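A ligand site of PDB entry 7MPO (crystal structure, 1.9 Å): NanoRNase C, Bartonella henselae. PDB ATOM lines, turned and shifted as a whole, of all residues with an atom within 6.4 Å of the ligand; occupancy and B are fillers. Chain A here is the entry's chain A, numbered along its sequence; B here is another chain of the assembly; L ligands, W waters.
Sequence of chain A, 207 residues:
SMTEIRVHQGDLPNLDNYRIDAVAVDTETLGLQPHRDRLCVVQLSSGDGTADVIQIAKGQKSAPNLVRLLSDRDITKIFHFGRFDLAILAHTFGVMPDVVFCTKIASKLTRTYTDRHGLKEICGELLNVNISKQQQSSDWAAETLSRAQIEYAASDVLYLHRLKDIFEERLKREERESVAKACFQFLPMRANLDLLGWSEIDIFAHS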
ATOM      1  N   ASP A  26      20.285   6.278  21.859  1.00  0.00           N
ATOM      2  CA  ASP A  26      21.019   5.692  22.971  1.00  0.00           C
ATOM      3  C   ASP A  26      21.573   6.828  23.819  1.00  0.00           C
ATOM      4  O   ASP A  26      21.595   7.982  23.384  1.00  0.00           O
ATOM      5  CB  ASP A  26      22.146   4.779  22.466  1.00  0.00           C
ATOM      6  CG  ASP A  26      22.775   3.942  23.573  1.00  0.00           C
ATOM      7  OD1 ASP A  26      22.093   3.635  24.574  1.00  0.00           O
ATOM      8  OD2 ASP A  26      23.955   3.589  23.419  1.00  0.00           O
ATOM      9  N   THR A  27      21.986   6.502  25.053  1.00  0.00           N
ATOM     10  CA  THR A  27      22.634   7.459  25.941  1.00  0.00           C
ATOM     11  C   THR A  27      23.959   6.903  26.435  1.00  0.00           C
ATOM     12  O   THR A  27      24.175   5.685  26.450  1.00  0.00           O
ATOM     13  CB  THR A  27      21.770   7.824  27.175  1.00  0.00           C
ATOM     14  OG1 THR A  27      21.566   6.668  28.000  1.00  0.00           O
ATOM     15  CG2 THR A  27      20.432   8.382  26.734  1.00  0.00           C
ATOM     16  N   GLU A  28      24.853   7.809  26.836  1.00  0.00           N
ATOM     17  CA  GLU A  28      25.993   7.454  27.664  1.00  0.00           C
ATOM     18  C   GLU A  28      25.999   8.362  28.889  1.00  0.00           C
ATOM     19  O   GLU A  28      25.612   9.539  28.814  1.00  0.00           O
ATOM     20  CB  GLU A  28      27.337   7.587  26.940  1.00  0.00           C
ATOM     21  CG  GLU A  28      27.454   6.766  25.642  1.00  0.00           C
ATOM     22  CD  GLU A  28      27.211   5.280  25.846  1.00  0.00           C
ATOM     23  OE1 GLU A  28      27.347   4.771  26.987  1.00  0.00           O
ATOM     24  OE2 GLU A  28      26.857   4.608  24.846  1.00  0.00           O
ATOM     25  N   LEU A  32      25.149   3.897  36.144  1.00  0.00           N
ATOM     26  CA  LEU A  32      23.787   3.383  36.030  1.00  0.00           C
ATOM     27  C   LEU A  32      22.829   3.969  37.063  1.00  0.00           C
ATOM     28  O   LEU A  32      21.689   3.498  37.150  1.00  0.00           O
ATOM     29  CB  LEU A  32      23.791   1.862  36.130  1.00  0.00           C
ATOM     30  CG  LEU A  32      24.660   1.207  35.047  1.00  0.00           C
ATOM     31  CD1 LEU A  32      24.651  -0.315  35.162  1.00  0.00           C
ATOM     32  CD2 LEU A  32      24.181   1.659  33.674  1.00  0.00           C
ATOM     33  N   GLN A  43      22.928   9.794  21.635  1.00  0.00           N
ATOM     34  CA  GLN A  43      23.209   9.403  20.253  1.00  0.00           C
ATOM     35  C   GLN A  43      21.902   9.164  19.514  1.00  0.00           C
ATOM     36  O   GLN A  43      20.947   8.607  20.064  1.00  0.00           O
ATOM     37  CB  GLN A  43      24.094   8.140  20.196  1.00  0.00           C
ATOM     38  CG  GLN A  43      25.371   8.213  21.035  1.00  0.00           C
ATOM     39  CD  GLN A  43      25.250   7.470  22.359  1.00  0.00           C
ATOM     40  OE1 GLN A  43      24.979   8.077  23.391  1.00  0.00           O
ATOM     41  NE2 GLN A  43      25.417   6.163  22.328  1.00  0.00           N
ATOM     42  N   HIS A  80      17.823   0.180  22.514  1.00  0.00           N
ATOM     43  CA  HIS A  80      18.175  -1.126  23.068  1.00  0.00           C
ATOM     44  C   HIS A  80      18.281  -0.979  24.582  1.00  0.00           C
ATOM     45  O   HIS A  80      19.133  -0.238  25.074  1.00  0.00           O
ATOM     46  CB  HIS A  80      19.479  -1.688  22.494  1.00  0.00           C
ATOM     47  CG  HIS A  80      19.830  -3.018  23.083  1.00  0.00           C
ATOM     48  ND1 HIS A  80      19.278  -4.197  22.638  1.00  0.00           N
ATOM     49  CD2 HIS A  80      20.602  -3.351  24.150  1.00  0.00           C
ATOM     50  CE1 HIS A  80      19.722  -5.203  23.370  1.00  0.00           C
ATOM     51  NE2 HIS A  80      20.532  -4.714  24.297  1.00  0.00           N
ATOM     52  N   PHE A  81      17.426  -1.699  25.306  1.00  0.00           N
ATOM     53  CA  PHE A  81      17.220  -1.466  26.742  1.00  0.00           C
ATOM     54  C   PHE A  81      16.810  -0.014  27.007  1.00  0.00           C
ATOM     55  O   PHE A  81      17.450   0.720  27.764  1.00  0.00           O
ATOM     56  CB  PHE A  81      18.436  -1.878  27.585  1.00  0.00           C
ATOM     57  CG  PHE A  81      18.105  -2.118  29.040  1.00  0.00           C
ATOM     58  CD1 PHE A  81      17.089  -3.001  29.395  1.00  0.00           C
ATOM     59  CD2 PHE A  81      18.794  -1.454  30.044  1.00  0.00           C
ATOM     60  CE1 PHE A  81      16.768  -3.230  30.720  1.00  0.00           C
ATOM     61  CE2 PHE A  81      18.496  -1.670  31.387  1.00  0.00           C
ATOM     62  CZ  PHE A  81      17.474  -2.565  31.724  1.00  0.00           C
ATOM     63  N   PHE A  84      16.503   1.945  30.592  1.00  0.00           N
ATOM     64  CA  PHE A  84      17.463   2.855  31.198  1.00  0.00           C
ATOM     65  C   PHE A  84      17.475   4.203  30.485  1.00  0.00           C
ATOM     66  O   PHE A  84      17.443   5.260  31.139  1.00  0.00           O
ATOM     67  CB  PHE A  84      18.871   2.250  31.219  1.00  0.00           C
ATOM     68  CG  PHE A  84      19.892   3.219  31.737  1.00  0.00           C
ATOM     69  CD1 PHE A  84      20.019   3.443  33.099  1.00  0.00           C
ATOM     70  CD2 PHE A  84      20.642   3.993  30.850  1.00  0.00           C
ATOM     71  CE1 PHE A  84      20.937   4.376  33.597  1.00  0.00           C
ATOM     72  CE2 PHE A  84      21.561   4.935  31.337  1.00  0.00           C
ATOM     73  CZ  PHE A  84      21.699   5.122  32.716  1.00  0.00           C
ATOM     74  N   ASP A  85      17.539   4.200  29.154  1.00  0.00           N
ATOM     75  CA  ASP A  85      17.611   5.459  28.415  1.00  0.00           C
ATOM     76  C   ASP A  85      16.434   6.359  28.728  1.00  0.00           C
ATOM     77  O   ASP A  85      16.591   7.575  28.911  1.00  0.00           O
ATOM     78  CB  ASP A  85      17.687   5.173  26.912  1.00  0.00           C
ATOM     79  CG  ASP A  85      18.900   4.334  26.556  1.00  0.00           C
ATOM     80  OD1 ASP A  85      19.989   4.606  27.106  1.00  0.00           O
ATOM     81  OD2 ASP A  85      18.780   3.395  25.747  1.00  0.00           O
ATOM     82  N   LYS A 104      15.775  -4.956  23.130  1.00  0.00           N
ATOM     83  CA  LYS A 104      16.005  -5.979  24.164  1.00  0.00           C
ATOM     84  C   LYS A 104      14.709  -6.703  24.510  1.00  0.00           C
ATOM     85  O   LYS A 104      14.675  -7.936  24.560  1.00  0.00           O
ATOM     86  CB  LYS A 104      16.621  -5.367  25.423  1.00  0.00           C
ATOM     87  CG  LYS A 104      16.467  -6.286  26.640  1.00  0.00           C
ATOM     88  CD  LYS A 104      17.623  -6.205  27.602  1.00  0.00           C
ATOM     89  CE  LYS A 104      18.910  -6.413  26.862  1.00  0.00           C
ATOM     90  NZ  LYS A 104      19.980  -7.009  27.675  1.00  0.00           N
ATOM     91  N   HIS A 117      20.792 -11.605  25.294  1.00  0.00           N
ATOM     92  CA  HIS A 117      19.973 -10.560  24.683  1.00  0.00           C
ATOM     93  C   HIS A 117      20.673  -9.203  24.677  1.00  0.00           C
ATOM     94  O   HIS A 117      20.005  -8.168  24.624  1.00  0.00           O
ATOM     95  CB  HIS A 117      18.614 -10.471  25.381  1.00  0.00           C
ATOM     96  CG  HIS A 117      17.862 -11.777  25.376  1.00  0.00           C
ATOM     97  ND1 HIS A 117      17.138 -12.208  24.293  1.00  0.00           N
ATOM     98  CD2 HIS A 117      17.766 -12.749  26.316  1.00  0.00           C
ATOM     99  CE1 HIS A 117      16.603 -13.393  24.570  1.00  0.00           C
ATOM    100  NE2 HIS A 117      16.977 -13.748  25.783  1.00  0.00           N
ATOM    101  N   GLY A 118      21.994  -9.181  24.722  1.00  0.00           N
ATOM    102  CA  GLY A 118      22.695  -7.913  24.594  1.00  0.00           C
ATOM    103  C   GLY A 118      22.831  -7.478  23.149  1.00  0.00           C
ATOM    104  O   GLY A 118      22.639  -8.252  22.212  1.00  0.00           O
ATOM    105  N   LEU A 119      23.187  -6.206  22.971  1.00  0.00           N
ATOM    106  CA  LEU A 119      23.214  -5.633  21.620  1.00  0.00           C
ATOM    107  C   LEU A 119      24.304  -6.260  20.761  1.00  0.00           C
ATOM    108  O   LEU A 119      24.095  -6.479  19.565  1.00  0.00           O
ATOM    109  CB  LEU A 119      23.405  -4.110  21.709  1.00  0.00           C
ATOM    110  CG  LEU A 119      23.348  -3.397  20.359  1.00  0.00           C
ATOM    111  CD1 LEU A 119      21.991  -3.580  19.700  1.00  0.00           C
ATOM    112  CD2 LEU A 119      23.652  -1.930  20.541  1.00  0.00           C
ATOM    113  N   LYS A 120      25.464  -6.538  21.360  1.00  0.00           N
ATOM    114  CA  LYS A 120      26.550  -7.167  20.611  1.00  0.00           C
ATOM    115  C   LYS A 120      26.132  -8.542  20.084  1.00  0.00           C
ATOM    116  O   LYS A 120      26.397  -8.876  18.925  1.00  0.00           O
ATOM    117  CB  LYS A 120      27.788  -7.285  21.514  1.00  0.00           C
ATOM    118  CG  LYS A 120      28.958  -8.045  20.892  1.00  0.00           C
ATOM    119  CD  LYS A 120      30.139  -8.100  21.872  1.00  0.00           C
ATOM    120  CE  LYS A 120      31.272  -8.940  21.341  1.00  0.00           C
ATOM    121  NZ  LYS A 120      31.754  -8.391  20.046  1.00  0.00           N
ATOM    122  N   GLU A 121      25.470  -9.339  20.924  1.00  0.00           N
ATOM    123  CA  GLU A 121      25.046 -10.675  20.511  1.00  0.00           C
ATOM    124  C   GLU A 121      23.973 -10.601  19.426  1.00  0.00           C
ATOM    125  O   GLU A 121      24.013 -11.352  18.443  1.00  0.00           O
ATOM    126  CB  GLU A 121      24.531 -11.438  21.732  1.00  0.00           C
ATOM    127  CG  GLU A 121      25.588 -11.814  22.785  1.00  0.00           C
ATOM    128  CD  GLU A 121      26.475 -10.651  23.245  1.00  0.00           C
ATOM    129  OE1 GLU A 121      27.703 -10.752  23.054  1.00  0.00           O
ATOM    130  OE2 GLU A 121      25.946  -9.636  23.778  1.00  0.00           O
ATOM    131  N   LYS A 133      32.919  -3.667  22.632  1.00  0.00           N
ATOM    132  CA  LYS A 133      32.466  -3.098  23.900  1.00  0.00           C
ATOM    133  C   LYS A 133      33.586  -2.405  24.668  1.00  0.00           C
ATOM    134  O   LYS A 133      33.337  -1.918  25.780  1.00  0.00           O
ATOM    135  CB  LYS A 133      31.848  -4.182  24.781  1.00  0.00           C
ATOM    136  CG  LYS A 133      30.678  -4.930  24.145  1.00  0.00           C
ATOM    137  CD  LYS A 133      29.462  -4.025  23.986  1.00  0.00           C
ATOM    138  CE  LYS A 133      28.741  -3.829  25.313  1.00  0.00           C
ATOM    139  NZ  LYS A 133      28.447  -5.130  25.990  1.00  0.00           N
ATOM    140  N   GLN A 136      32.919   0.924  26.397  1.00  0.00           N
ATOM    141  CA  GLN A 136      31.799   1.061  27.334  1.00  0.00           C
ATOM    142  C   GLN A 136      32.262   1.606  28.671  1.00  0.00           C
ATOM    143  O   GLN A 136      31.647   2.524  29.229  1.00  0.00           O
ATOM    144  CB  GLN A 136      31.109  -0.297  27.512  1.00  0.00           C
ATOM    145  CG  GLN A 136      29.736  -0.209  28.148  1.00  0.00           C
ATOM    146  CD  GLN A 136      28.961  -1.509  27.975  1.00  0.00           C
ATOM    147  OE1 GLN A 136      29.509  -2.594  28.170  1.00  0.00           O
ATOM    148  NE2 GLN A 136      27.692  -1.402  27.591  1.00  0.00           N
ATOM    149  N   TYR A 152      32.182   4.061  19.177  1.00  0.00           N
ATOM    150  CA  TYR A 152      31.379   3.171  19.999  1.00  0.00           C
ATOM    151  C   TYR A 152      29.980   3.729  20.196  1.00  0.00           C
ATOM    152  O   TYR A 152      28.972   3.040  19.969  1.00  0.00           O
ATOM    153  CB  TYR A 152      32.045   2.930  21.361  1.00  0.00           C
ATOM    154  CG  TYR A 152      31.139   2.117  22.251  1.00  0.00           C
ATOM    155  CD1 TYR A 152      30.390   2.717  23.255  1.00  0.00           C
ATOM    156  CD2 TYR A 152      30.969   0.757  22.017  1.00  0.00           C
ATOM    157  CE1 TYR A 152      29.533   1.963  24.050  1.00  0.00           C
ATOM    158  CE2 TYR A 152      30.124  -0.004  22.808  1.00  0.00           C
ATOM    159  CZ  TYR A 152      29.403   0.604  23.810  1.00  0.00           C
ATOM    160  OH  TYR A 152      28.553  -0.155  24.584  1.00  0.00           O
ATOM    161  N   ASP A 156      26.094   2.139  18.738  1.00  0.00           N
ATOM    162  CA  ASP A 156      24.910   1.745  19.482  1.00  0.00           C
ATOM    163  C   ASP A 156      23.614   2.121  18.777  1.00  0.00           C
ATOM    164  O   ASP A 156      22.579   1.501  19.056  1.00  0.00           O
ATOM    165  CB  ASP A 156      24.937   2.361  20.883  1.00  0.00           C
ATOM    166  CG  ASP A 156      25.939   1.673  21.836  1.00  0.00           C
ATOM    167  OD1 ASP A 156      26.256   0.476  21.628  1.00  0.00           O
ATOM    168  OD2 ASP A 156      26.410   2.330  22.786  1.00  0.00           O
ATOM    169  N   HIS B 206      17.166  -6.279  32.471  1.00  0.00           N
ATOM    170  CA  HIS B 206      18.289  -6.302  31.536  1.00  0.00           C
ATOM    171  C   HIS B 206      18.751  -7.725  31.276  1.00  0.00           C
ATOM    172  O   HIS B 206      19.028  -8.110  30.133  1.00  0.00           O
ATOM    173  CB  HIS B 206      19.462  -5.474  32.080  1.00  0.00           C
ATOM    174  CG  HIS B 206      20.721  -5.635  31.286  1.00  0.00           C
ATOM    175  ND1 HIS B 206      21.591  -6.679  31.493  1.00  0.00           N
ATOM    176  CD2 HIS B 206      21.235  -4.904  30.275  1.00  0.00           C
ATOM    177  CE1 HIS B 206      22.600  -6.577  30.635  1.00  0.00           C
ATOM    178  NE2 HIS B 206      22.404  -5.507  29.885  1.00  0.00           N
ATOM    179  N   SER B 207      18.878  -8.518  32.331  1.00  0.00           N
ATOM    180  CA  SER B 207      19.316  -9.906  32.233  1.00  0.00           C
ATOM    181  C   SER B 207      18.814 -10.708  33.410  1.00  0.00           C
ATOM    182  O   SER B 207      18.790 -11.940  33.366  1.00  0.00           O
ATOM    183  CB  SER B 207      20.840  -9.990  32.157  1.00  0.00           C
ATOM    184  OG  SER B 207      21.430  -9.107  33.069  1.00  0.00           O
ATOM    185  OXT SER B 207      18.417 -10.138  34.430  1.00  0.00           O
HETATM  186  P1  LIG L   1      25.230   0.979  25.866  1.00  0.00           P
HETATM  187  O1  LIG L   1      26.668   0.612  26.175  1.00  0.00           O
HETATM  188  O2  LIG L   1      25.127   2.443  25.507  1.00  0.00           O
HETATM  189  O3  LIG L   1      24.676   0.129  24.744  1.00  0.00           O
HETATM  190  P2  LIG L   1      23.216  -4.673  26.545  1.00  0.00           P
HETATM  191  O4  LIG L   1      24.017  -5.212  27.701  1.00  0.00           O
HETATM  192  O5  LIG L   1      21.851  -5.319  26.554  1.00  0.00           O
HETATM  193  O6  LIG L   1      23.914  -4.884  25.224  1.00  0.00           O
HETATM  194  O7  LIG L   1      23.063  -3.016  26.648  1.00  0.00           O
HETATM  195  C1  LIG L   1      22.399  -2.405  27.706  1.00  0.00           C
HETATM  196  C2  LIG L   1      22.667  -0.876  27.577  1.00  0.00           C
HETATM  197  O8  LIG L   1      22.103  -0.266  28.585  1.00  0.00           O
HETATM  198  C3  LIG L   1      24.164  -0.540  27.725  1.00  0.00           C
HETATM  199  O9  LIG L   1      24.354   0.706  27.240  1.00  0.00           O
HETATM  200  C4  LIG L   1      24.340  -0.493  29.258  1.00  0.00           C
HETATM  201  O10 LIG L   1      25.544   0.333  29.586  1.00  0.00           O
HETATM  202  C5  LIG L   1      23.262   0.118  29.656  1.00  0.00           C
HETATM  203  N1  LIG L   1      22.688  -0.308  30.905  1.00  0.00           N
HETATM  204  C6  LIG L   1      21.816   0.445  31.590  1.00  0.00           C
HETATM  205  N2  LIG L   1      21.426  -0.247  32.675  1.00  0.00           N
HETATM  206  C7  LIG L   1      22.048  -1.432  32.639  1.00  0.00           C
HETATM  207  C8  LIG L   1      21.996  -2.482  33.516  1.00  0.00           C
HETATM  208  N3  LIG L   1      21.186  -2.504  34.714  1.00  0.00           N
HETATM  209  N4  LIG L   1      22.700  -3.577  33.286  1.00  0.00           N
HETATM  210  C9  LIG L   1      23.490  -3.642  32.191  1.00  0.00           C
HETATM  211  N5  LIG L   1      23.536  -2.607  31.320  1.00  0.00           N
HETATM  212  C10 LIG L   1      22.809  -1.491  31.547  1.00  0.00           C
HETATM  213  O   HOH W   1      26.346  -3.873  28.593  1.00  0.00           O
HETATM  214  O   HOH W   2      25.093  -2.402  24.311  1.00  0.00           O
HETATM  215  O   HOH W   3      25.002  -7.401  27.549  1.00  0.00           O
HETATM  216  O   HOH W   4      26.155  -5.872  24.213  1.00  0.00           O
HETATM  217  O   HOH W   5      19.758   0.286  34.877  1.00  0.00           O
HETATM  218  O   HOH W   6      22.123   0.421  24.152  1.00  0.00           O
HETATM  219  O   HOH W   7      28.293   2.248  27.645  1.00  0.00           O
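O1 of the ligand lies within hydrogen-bond range of OH of Tyr 152, at 2.6 Å. The side-chain carboxylate (OD2) of Asp 26 lies close to an oxygen (O2) of the ligand (2.7 Å). NE2 of Gln 136 lies within hydrogen-bond range of O1 of the ligand. An oxygen (O5) of the ligand is in hydrogen-bond range of a ring nitrogen (NE2) of His 80. O6 of the ligand sits at hydrogen-bond distance from N of Leu 119 (2.7 Å). An oxygen (O4) of the ligand sits at hydrogen-bond distance from a ring nitrogen (NE2) of His 206 of chain B, at 2.7 Å. An oxygen (O5) of the ligand is in salt-bridge range of the side-chain amino group of Lys 104. The side-chain carboxylate (OE2) of Glu 28 sits close to an oxygen (O2) of the ligand. OD2 of Asp 156 lies close to O2 of the ligand (3.0 Å).
The side-chain hydroxyl (OH) of Tyr 152 sits at hydrogen-bond distance from the side-chain amide nitrogen (NE2) of Gln 136. O of Asp 26 is in hydrogen-bond range of N of Gln 43, 2.8 Å away. A ring nitrogen (NE2) of His 80 lies within hydrogen-bond range of the backbone NH of Leu 119 (3.3 Å). The backbone carbonyl oxygen (O) of His 206 of chain B lies within hydrogen-bond range of the side-chain amino group (NZ) of Lys 104 (2.9 Å). The side-chain hydroxyl of Ser 207 of chain B sits at hydrogen-bond distance from a ring nitrogen (ND1) of His 206 of chain B (2.9 Å). NZ of Lys 104 lies close to O of His 117 (3.3 Å). The side-chain carboxylate of Glu 28 is in hydrogen-bond range of the side-chain amide nitrogen of Gln 43. The side-chain hydroxyl of Thr 27 sits at hydrogen-bond distance from the side-chain carboxylate of Asp 85 (2.7 Å).
Residues that only touch the ligand: Thr 27 (3.5 Å), Leu 32 (3.4 Å), Phe 81 (3.5 Å), Phe 84 (3.4 Å), His 117 (3.9 Å) and Gly 118 (3.3 Å). Hydrophobic or aromatic side chains that line the ligand: Leu 32, His 80, Phe 81, Phe 84, Leu 119, Tyr 152 and His 206 of chain B. 15 residues have an atom within 4 Å of the ligand: Asp 26, Thr 27, Glu 28, Leu 32, His 80, Phe 81, Phe 84, Lys 104, His 117, Gly 118, Leu 119, Gln 136, Tyr 152, Asp 156 and His 206 of chain B. The nearest printed residue that does not touch the ligand is Lys 120 (4.5 Å).
Water W6 lies within hydrogen-bond range of O3 of the ligand (2.6 Å), O of His 80 (3.2 Å) and OD1 of Asp 26 (3.2 Å). Water W7 lies within hydrogen-bond range of an oxygen (O1) of the ligand (2.7 Å) and the side-chain carboxylate (OE1) of Glu 28 (2.8 Å). Water W1 bridges O4 of the ligand and NE2 of Gln 136.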
